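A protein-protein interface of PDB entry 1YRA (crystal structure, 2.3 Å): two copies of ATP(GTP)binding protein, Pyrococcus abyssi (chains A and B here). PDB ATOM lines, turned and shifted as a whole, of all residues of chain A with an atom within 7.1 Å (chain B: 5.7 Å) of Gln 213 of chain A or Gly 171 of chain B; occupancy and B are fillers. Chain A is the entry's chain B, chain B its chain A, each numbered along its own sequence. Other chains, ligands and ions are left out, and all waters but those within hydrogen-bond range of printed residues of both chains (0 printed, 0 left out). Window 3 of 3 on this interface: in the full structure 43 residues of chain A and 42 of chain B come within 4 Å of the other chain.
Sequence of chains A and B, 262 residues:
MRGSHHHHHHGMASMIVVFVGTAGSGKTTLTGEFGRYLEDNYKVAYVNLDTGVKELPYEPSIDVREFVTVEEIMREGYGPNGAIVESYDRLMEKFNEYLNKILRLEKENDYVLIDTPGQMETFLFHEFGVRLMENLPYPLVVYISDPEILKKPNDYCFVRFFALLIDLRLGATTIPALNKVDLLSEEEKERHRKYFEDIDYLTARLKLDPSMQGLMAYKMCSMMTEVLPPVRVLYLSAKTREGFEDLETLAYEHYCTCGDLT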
ATOM      1  N   LYS A 152      -3.669  17.209  -7.945  1.00  0.00           N
ATOM      2  CA  LYS A 152      -3.766  18.013  -6.722  1.00  0.00           C
ATOM      3  C   LYS A 152      -5.077  17.731  -5.973  1.00  0.00           C
ATOM      4  O   LYS A 152      -6.002  17.180  -6.546  1.00  0.00           O
ATOM      5  CB  LYS A 152      -3.647  19.496  -7.066  1.00  0.00           C
ATOM      6  CG  LYS A 152      -4.349  19.875  -8.363  1.00  0.00           C
ATOM      7  CD  LYS A 152      -4.998  21.265  -8.295  1.00  0.00           C
ATOM      8  CE  LYS A 152      -6.206  21.355  -9.238  1.00  0.00           C
ATOM      9  NZ  LYS A 152      -5.842  21.524 -10.676  1.00  0.00           N
ATOM     10  N   ASN A 154      -7.754  19.265  -5.105  1.00  0.00           N
ATOM     11  CA  ASN A 154      -8.962  19.686  -5.794  1.00  0.00           C
ATOM     12  C   ASN A 154      -9.461  18.675  -6.861  1.00  0.00           C
ATOM     13  O   ASN A 154     -10.666  18.558  -7.089  1.00  0.00           O
ATOM     14  CB  ASN A 154      -8.728  21.069  -6.410  1.00  0.00           C
ATOM     15  CG  ASN A 154      -8.910  22.210  -5.395  1.00  0.00           C
ATOM     16  OD1 ASN A 154      -9.417  21.995  -4.293  1.00  0.00           O
ATOM     17  ND2 ASN A 154      -8.507  23.434  -5.777  1.00  0.00           N
ATOM     18  N   LEU A 206      -8.633  20.174   1.958  1.00  0.00           N
ATOM     19  CA  LEU A 206      -9.176  21.257   1.120  1.00  0.00           C
ATOM     20  C   LEU A 206      -9.433  22.497   1.963  1.00  0.00           C
ATOM     21  O   LEU A 206      -9.343  23.636   1.482  1.00  0.00           O
ATOM     22  CB  LEU A 206     -10.479  20.821   0.455  1.00  0.00           C
ATOM     23  CG  LEU A 206     -10.439  19.586  -0.446  1.00  0.00           C
ATOM     24  CD1 LEU A 206     -11.841  19.257  -0.920  1.00  0.00           C
ATOM     25  CD2 LEU A 206      -9.444  19.770  -1.631  1.00  0.00           C
ATOM     26  N   ASP A 209      -6.792  25.242   2.217  1.00  0.00           N
ATOM     27  CA  ASP A 209      -6.536  26.060   1.035  1.00  0.00           C
ATOM     28  C   ASP A 209      -7.509  27.236   1.016  1.00  0.00           C
ATOM     29  O   ASP A 209      -8.689  27.061   0.756  1.00  0.00           O
ATOM     30  CB  ASP A 209      -6.645  25.207  -0.246  1.00  0.00           C
ATOM     31  CG  ASP A 209      -6.448  26.028  -1.526  1.00  0.00           C
ATOM     32  OD1 ASP A 209      -6.539  25.471  -2.640  1.00  0.00           O
ATOM     33  OD2 ASP A 209      -6.225  27.247  -1.414  1.00  0.00           O
ATOM     34  N   PRO A 210      -7.009  28.447   1.302  1.00  0.00           N
ATOM     35  CA  PRO A 210      -7.868  29.618   1.477  1.00  0.00           C
ATOM     36  C   PRO A 210      -8.276  30.316   0.167  1.00  0.00           C
ATOM     37  O   PRO A 210      -8.957  31.350   0.197  1.00  0.00           O
ATOM     38  CB  PRO A 210      -7.008  30.557   2.337  1.00  0.00           C
ATOM     39  CG  PRO A 210      -5.597  30.158   2.077  1.00  0.00           C
ATOM     40  CD  PRO A 210      -5.580  28.773   1.469  1.00  0.00           C
ATOM     41  N   SER A 211      -7.866  29.761  -0.966  1.00  0.00           N
ATOM     42  CA  SER A 211      -8.234  30.348  -2.248  1.00  0.00           C
ATOM     43  C   SER A 211      -9.689  30.045  -2.600  1.00  0.00           C
ATOM     44  O   SER A 211     -10.320  29.178  -1.984  1.00  0.00           O
ATOM     45  CB  SER A 211      -7.313  29.844  -3.356  1.00  0.00           C
ATOM     46  OG  SER A 211      -7.301  28.430  -3.378  1.00  0.00           O
ATOM     47  N   MET A 212     -10.206  30.787  -3.579  1.00  0.00           N
ATOM     48  CA  MET A 212     -11.567  30.622  -4.068  1.00  0.00           C
ATOM     49  C   MET A 212     -11.846  29.175  -4.439  1.00  0.00           C
ATOM     50  O   MET A 212     -12.831  28.599  -3.988  1.00  0.00           O
ATOM     51  CB  MET A 212     -11.817  31.523  -5.277  1.00  0.00           C
ATOM     52  CG  MET A 212     -11.795  33.020  -4.972  1.00  0.00           C
ATOM     53  SD  MET A 212     -12.436  34.003  -6.352  1.00  0.00           S
ATOM     54  CE  MET A 212     -11.870  35.645  -5.888  1.00  0.00           C
ATOM     55  N   GLN A 213     -10.960  28.585  -5.233  1.00  0.00           N
ATOM     56  CA  GLN A 213     -11.135  27.224  -5.699  1.00  0.00           C
ATOM     57  C   GLN A 213     -11.120  26.244  -4.512  1.00  0.00           C
ATOM     58  O   GLN A 213     -11.979  25.360  -4.404  1.00  0.00           O
ATOM     59  CB  GLN A 213     -10.043  26.882  -6.726  1.00  0.00           C
ATOM     60  CG  GLN A 213     -10.578  26.420  -8.095  1.00  0.00           C
ATOM     61  CD  GLN A 213      -9.532  26.486  -9.208  1.00  0.00           C
ATOM     62  OE1 GLN A 213      -9.215  25.478  -9.846  1.00  0.00           O
ATOM     63  NE2 GLN A 213      -8.989  27.679  -9.445  1.00  0.00           N
ATOM     64  N   GLY A 214     -10.153  26.419  -3.613  1.00  0.00           N
ATOM     65  CA  GLY A 214     -10.022  25.542  -2.456  1.00  0.00           C
ATOM     66  C   GLY A 214     -11.242  25.631  -1.567  1.00  0.00           C
ATOM     67  O   GLY A 214     -11.700  24.629  -1.032  1.00  0.00           O
ATOM     68  N   LEU A 215     -11.756  26.848  -1.414  1.00  0.00           N
ATOM     69  CA  LEU A 215     -12.982  27.111  -0.659  1.00  0.00           C
ATOM     70  C   LEU A 215     -14.149  26.337  -1.244  1.00  0.00           C
ATOM     71  O   LEU A 215     -14.862  25.616  -0.531  1.00  0.00           O
ATOM     72  CB  LEU A 215     -13.322  28.595  -0.711  1.00  0.00           C
ATOM     73  CG  LEU A 215     -13.060  29.525   0.477  1.00  0.00           C
ATOM     74  CD1 LEU A 215     -11.857  29.156   1.301  1.00  0.00           C
ATOM     75  CD2 LEU A 215     -12.932  30.939  -0.035  1.00  0.00           C
ATOM     76  N   MET A 216     -14.337  26.489  -2.552  1.00  0.00           N
ATOM     77  CA  MET A 216     -15.466  25.873  -3.209  1.00  0.00           C
ATOM     78  C   MET A 216     -15.313  24.362  -3.227  1.00  0.00           C
ATOM     79  O   MET A 216     -16.281  23.648  -3.067  1.00  0.00           O
ATOM     80  CB  MET A 216     -15.653  26.424  -4.615  1.00  0.00           C
ATOM     81  CG  MET A 216     -17.035  26.126  -5.159  1.00  0.00           C
ATOM     82  SD  MET A 216     -17.030  26.111  -6.951  1.00  0.00           S
ATOM     83  CE  MET A 216     -16.305  27.713  -7.267  1.00  0.00           C
ATOM     84  N   ALA A 217     -14.093  23.880  -3.400  1.00  0.00           N
ATOM     85  CA  ALA A 217     -13.824  22.450  -3.328  1.00  0.00           C
ATOM     86  C   ALA A 217     -14.168  21.909  -1.943  1.00  0.00           C
ATOM     87  O   ALA A 217     -14.893  20.918  -1.810  1.00  0.00           O
ATOM     88  CB  ALA A 217     -12.366  22.163  -3.658  1.00  0.00           C
ATOM     89  N   TYR A 218     -13.619  22.558  -0.922  1.00  0.00           N
ATOM     90  CA  TYR A 218     -13.943  22.259   0.462  1.00  0.00           C
ATOM     91  C   TYR A 218     -15.450  22.178   0.678  1.00  0.00           C
ATOM     92  O   TYR A 218     -15.928  21.275   1.327  1.00  0.00           O
ATOM     93  CB  TYR A 218     -13.346  23.315   1.410  1.00  0.00           C
ATOM     94  CG  TYR A 218     -13.807  23.132   2.843  1.00  0.00           C
ATOM     95  CD1 TYR A 218     -14.554  24.109   3.487  1.00  0.00           C
ATOM     96  CD2 TYR A 218     -13.519  21.964   3.538  1.00  0.00           C
ATOM     97  CE1 TYR A 218     -14.985  23.929   4.790  1.00  0.00           C
ATOM     98  CE2 TYR A 218     -13.941  21.778   4.824  1.00  0.00           C
ATOM     99  CZ  TYR A 218     -14.672  22.757   5.449  1.00  0.00           C
ATOM    100  OH  TYR A 218     -15.090  22.555   6.743  1.00  0.00           O
ATOM    101  N   LYS A 219     -16.187  23.141   0.135  1.00  0.00           N
ATOM    102  CA  LYS A 219     -17.634  23.190   0.286  1.00  0.00           C
ATOM    103  C   LYS A 219     -18.355  22.026  -0.419  1.00  0.00           C
ATOM    104  O   LYS A 219     -19.184  21.327   0.183  1.00  0.00           O
ATOM    105  CB  LYS A 219     -18.154  24.516  -0.255  1.00  0.00           C
ATOM    106  CG  LYS A 219     -18.184  25.648   0.767  1.00  0.00           C
ATOM    107  CD  LYS A 219     -17.767  26.981   0.143  1.00  0.00           C
ATOM    108  CE  LYS A 219     -18.384  27.185  -1.230  1.00  0.00           C
ATOM    109  NZ  LYS A 219     -17.890  28.446  -1.874  1.00  0.00           N
ATOM    110  N   MET A 220     -18.044  21.819  -1.694  1.00  0.00           N
ATOM    111  CA  MET A 220     -18.687  20.759  -2.450  1.00  0.00           C
ATOM    112  C   MET A 220     -18.350  19.428  -1.798  1.00  0.00           C
ATOM    113  O   MET A 220     -19.148  18.492  -1.791  1.00  0.00           O
ATOM    114  CB  MET A 220     -18.231  20.784  -3.912  1.00  0.00           C
ATOM    115  CG  MET A 220     -18.241  22.176  -4.515  1.00  0.00           C
ATOM    116  SD  MET A 220     -18.185  22.199  -6.310  1.00  0.00           S
ATOM    117  CE  MET A 220     -19.930  22.085  -6.702  1.00  0.00           C
ATOM    118  N   ILE B 166     -18.108  22.297 -13.260  1.00  0.00           N
ATOM    119  CA  ILE B 166     -17.319  22.903 -14.322  1.00  0.00           C
ATOM    120  C   ILE B 166     -16.543  24.088 -13.763  1.00  0.00           C
ATOM    121  O   ILE B 166     -15.364  24.287 -14.055  1.00  0.00           O
ATOM    122  CB  ILE B 166     -18.211  23.394 -15.496  1.00  0.00           C
ATOM    123  CG1 ILE B 166     -18.737  22.204 -16.308  1.00  0.00           C
ATOM    124  CG2 ILE B 166     -17.414  24.382 -16.353  1.00  0.00           C
ATOM    125  CD1 ILE B 166     -19.756  22.556 -17.377  1.00  0.00           C
ATOM    126  N   ASP B 167     -17.221  24.869 -12.937  1.00  0.00           N
ATOM    127  CA  ASP B 167     -16.608  26.019 -12.278  1.00  0.00           C
ATOM    128  C   ASP B 167     -15.445  25.572 -11.374  1.00  0.00           C
ATOM    129  O   ASP B 167     -14.390  26.219 -11.345  1.00  0.00           O
ATOM    130  CB  ASP B 167     -17.678  26.808 -11.500  1.00  0.00           C
ATOM    131  CG  ASP B 167     -17.132  28.056 -10.857  1.00  0.00           C
ATOM    132  OD1 ASP B 167     -15.925  28.066 -10.520  1.00  0.00           O
ATOM    133  OD2 ASP B 167     -17.914  29.038 -10.695  1.00  0.00           O
ATOM    134  N   LEU B 168     -15.620  24.448 -10.678  1.00  0.00           N
ATOM    135  CA  LEU B 168     -14.539  23.878  -9.882  1.00  0.00           C
ATOM    136  C   LEU B 168     -13.402  23.448 -10.799  1.00  0.00           C
ATOM    137  O   LEU B 168     -12.248  23.854 -10.625  1.00  0.00           O
ATOM    138  CB  LEU B 168     -15.029  22.664  -9.088  1.00  0.00           C
ATOM    139  CG  LEU B 168     -14.027  21.933  -8.188  1.00  0.00           C
ATOM    140  CD1 LEU B 168     -13.420  22.869  -7.101  1.00  0.00           C
ATOM    141  CD2 LEU B 168     -14.656  20.709  -7.510  1.00  0.00           C
ATOM    142  N   ARG B 169     -13.738  22.608 -11.775  1.00  0.00           N
ATOM    143  CA  ARG B 169     -12.736  21.992 -12.620  1.00  0.00           C
ATOM    144  C   ARG B 169     -11.874  23.035 -13.358  1.00  0.00           C
ATOM    145  O   ARG B 169     -10.640  22.964 -13.325  1.00  0.00           O
ATOM    146  CB  ARG B 169     -13.408  21.044 -13.600  1.00  0.00           C
ATOM    147  CG  ARG B 169     -12.453  20.387 -14.534  1.00  0.00           C
ATOM    148  CD  ARG B 169     -11.328  19.696 -13.780  1.00  0.00           C
ATOM    149  NE  ARG B 169     -10.654  18.787 -14.701  1.00  0.00           N
ATOM    150  CZ  ARG B 169      -9.532  18.120 -14.437  1.00  0.00           C
ATOM    151  NH1 ARG B 169      -8.924  18.256 -13.255  1.00  0.00           N
ATOM    152  NH2 ARG B 169      -9.031  17.312 -15.363  1.00  0.00           N
ATOM    153  N   LEU B 170     -12.525  24.020 -13.968  1.00  0.00           N
ATOM    154  CA  LEU B 170     -11.843  24.979 -14.830  1.00  0.00           C
ATOM    155  C   LEU B 170     -11.450  26.256 -14.090  1.00  0.00           C
ATOM    156  O   LEU B 170     -10.683  27.088 -14.610  1.00  0.00           O
ATOM    157  CB  LEU B 170     -12.720  25.325 -16.037  1.00  0.00           C
ATOM    158  CG  LEU B 170     -13.114  24.128 -16.898  1.00  0.00           C
ATOM    159  CD1 LEU B 170     -14.017  24.539 -18.065  1.00  0.00           C
ATOM    160  CD2 LEU B 170     -11.830  23.466 -17.402  1.00  0.00           C
ATOM    161  N   GLY B 171     -11.974  26.422 -12.880  1.00  0.00           N
ATOM    162  CA  GLY B 171     -11.565  27.555 -12.061  1.00  0.00           C
ATOM    163  C   GLY B 171     -11.971  28.849 -12.726  1.00  0.00           C
ATOM    164  O   GLY B 171     -11.208  29.799 -12.750  1.00  0.00           O
ATOM    165  N   ALA B 172     -13.192  28.875 -13.263  1.00  0.00           N
ATOM    166  CA  ALA B 172     -13.699  30.024 -14.001  1.00  0.00           C
ATOM    167  C   ALA B 172     -15.168  30.240 -13.694  1.00  0.00           C
ATOM    168  O   ALA B 172     -15.921  29.285 -13.521  1.00  0.00           O
ATOM    169  CB  ALA B 172     -13.496  29.835 -15.502  1.00  0.00           C
ATOM    170  N   THR B 173     -15.576  31.496 -13.604  1.00  0.00           N
ATOM    171  CA  THR B 173     -17.005  31.810 -13.470  1.00  0.00           C
ATOM    172  C   THR B 173     -17.795  31.083 -14.549  1.00  0.00           C
ATOM    173  O   THR B 173     -17.632  31.375 -15.731  1.00  0.00           O
ATOM    174  CB  THR B 173     -17.264  33.313 -13.633  1.00  0.00           C
ATOM    175  OG1 THR B 173     -16.411  34.034 -12.735  1.00  0.00           O
ATOM    176  CG2 THR B 173     -18.729  33.646 -13.337  1.00  0.00           C
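The backbone NH (N) of Ala 172 of chain B sits at hydrogen-bond distance from the backbone carbonyl oxygen (O) of Asp 167 of chain B (3.5 Å).
Among the printed residues, pairs that only touch across the chains: Gln 213 of chain A with Leu 168 of chain B (3.5 Å), Gln 213 of chain A with Gly 171 of chain B (3.7 Å), Met 216 of chain A with Asp 167 of chain B (3.3 Å) and Ala 217 of chain A with Leu 168 of chain B (3.7 Å).
Printed residues of chain B within 4 Å of Gln 213 of chain A: Leu 168 and Gly 171.
Printed residues of chain B within 4 Å of Met 216 of chain A: Asp 167 (3.3 Å).
Printed residues of chain B within 4 Å of Ala 217 of chain A: Leu 168.
Printed residues of chain A within 4 Å of Asp 167 of chain B: Met 216.
Of the printed residues of chain A, Leu 168 of chain B touches Gln 213 (3.5 Å) and Ala 217 (3.7 Å).
Of the printed residues of chain A, Gly 171 of chain B touches Gln 213 (3.7 Å).
The nearest residue of chain B that does not touch Gln 213 of chain A is Arg 169 of chain B (4.5 Å).
The nearest residue of chain A that does not touch Gly 171 of chain B is Met 216 of chain A (6.7 Å).
Of the 8 printed residues of chain B, 3 touch a printed residue of chain A.
Printed residues of chain B that touch a printed residue of chain A: Asp 167, Leu 168 and Gly 171.
Among the printed residues, 4 pairs touch across the chains.
No position is printed for both chains.
Of the 4 pairs that touch across the chains among the printed residues, none has its exchanged pair printed and touching as well.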
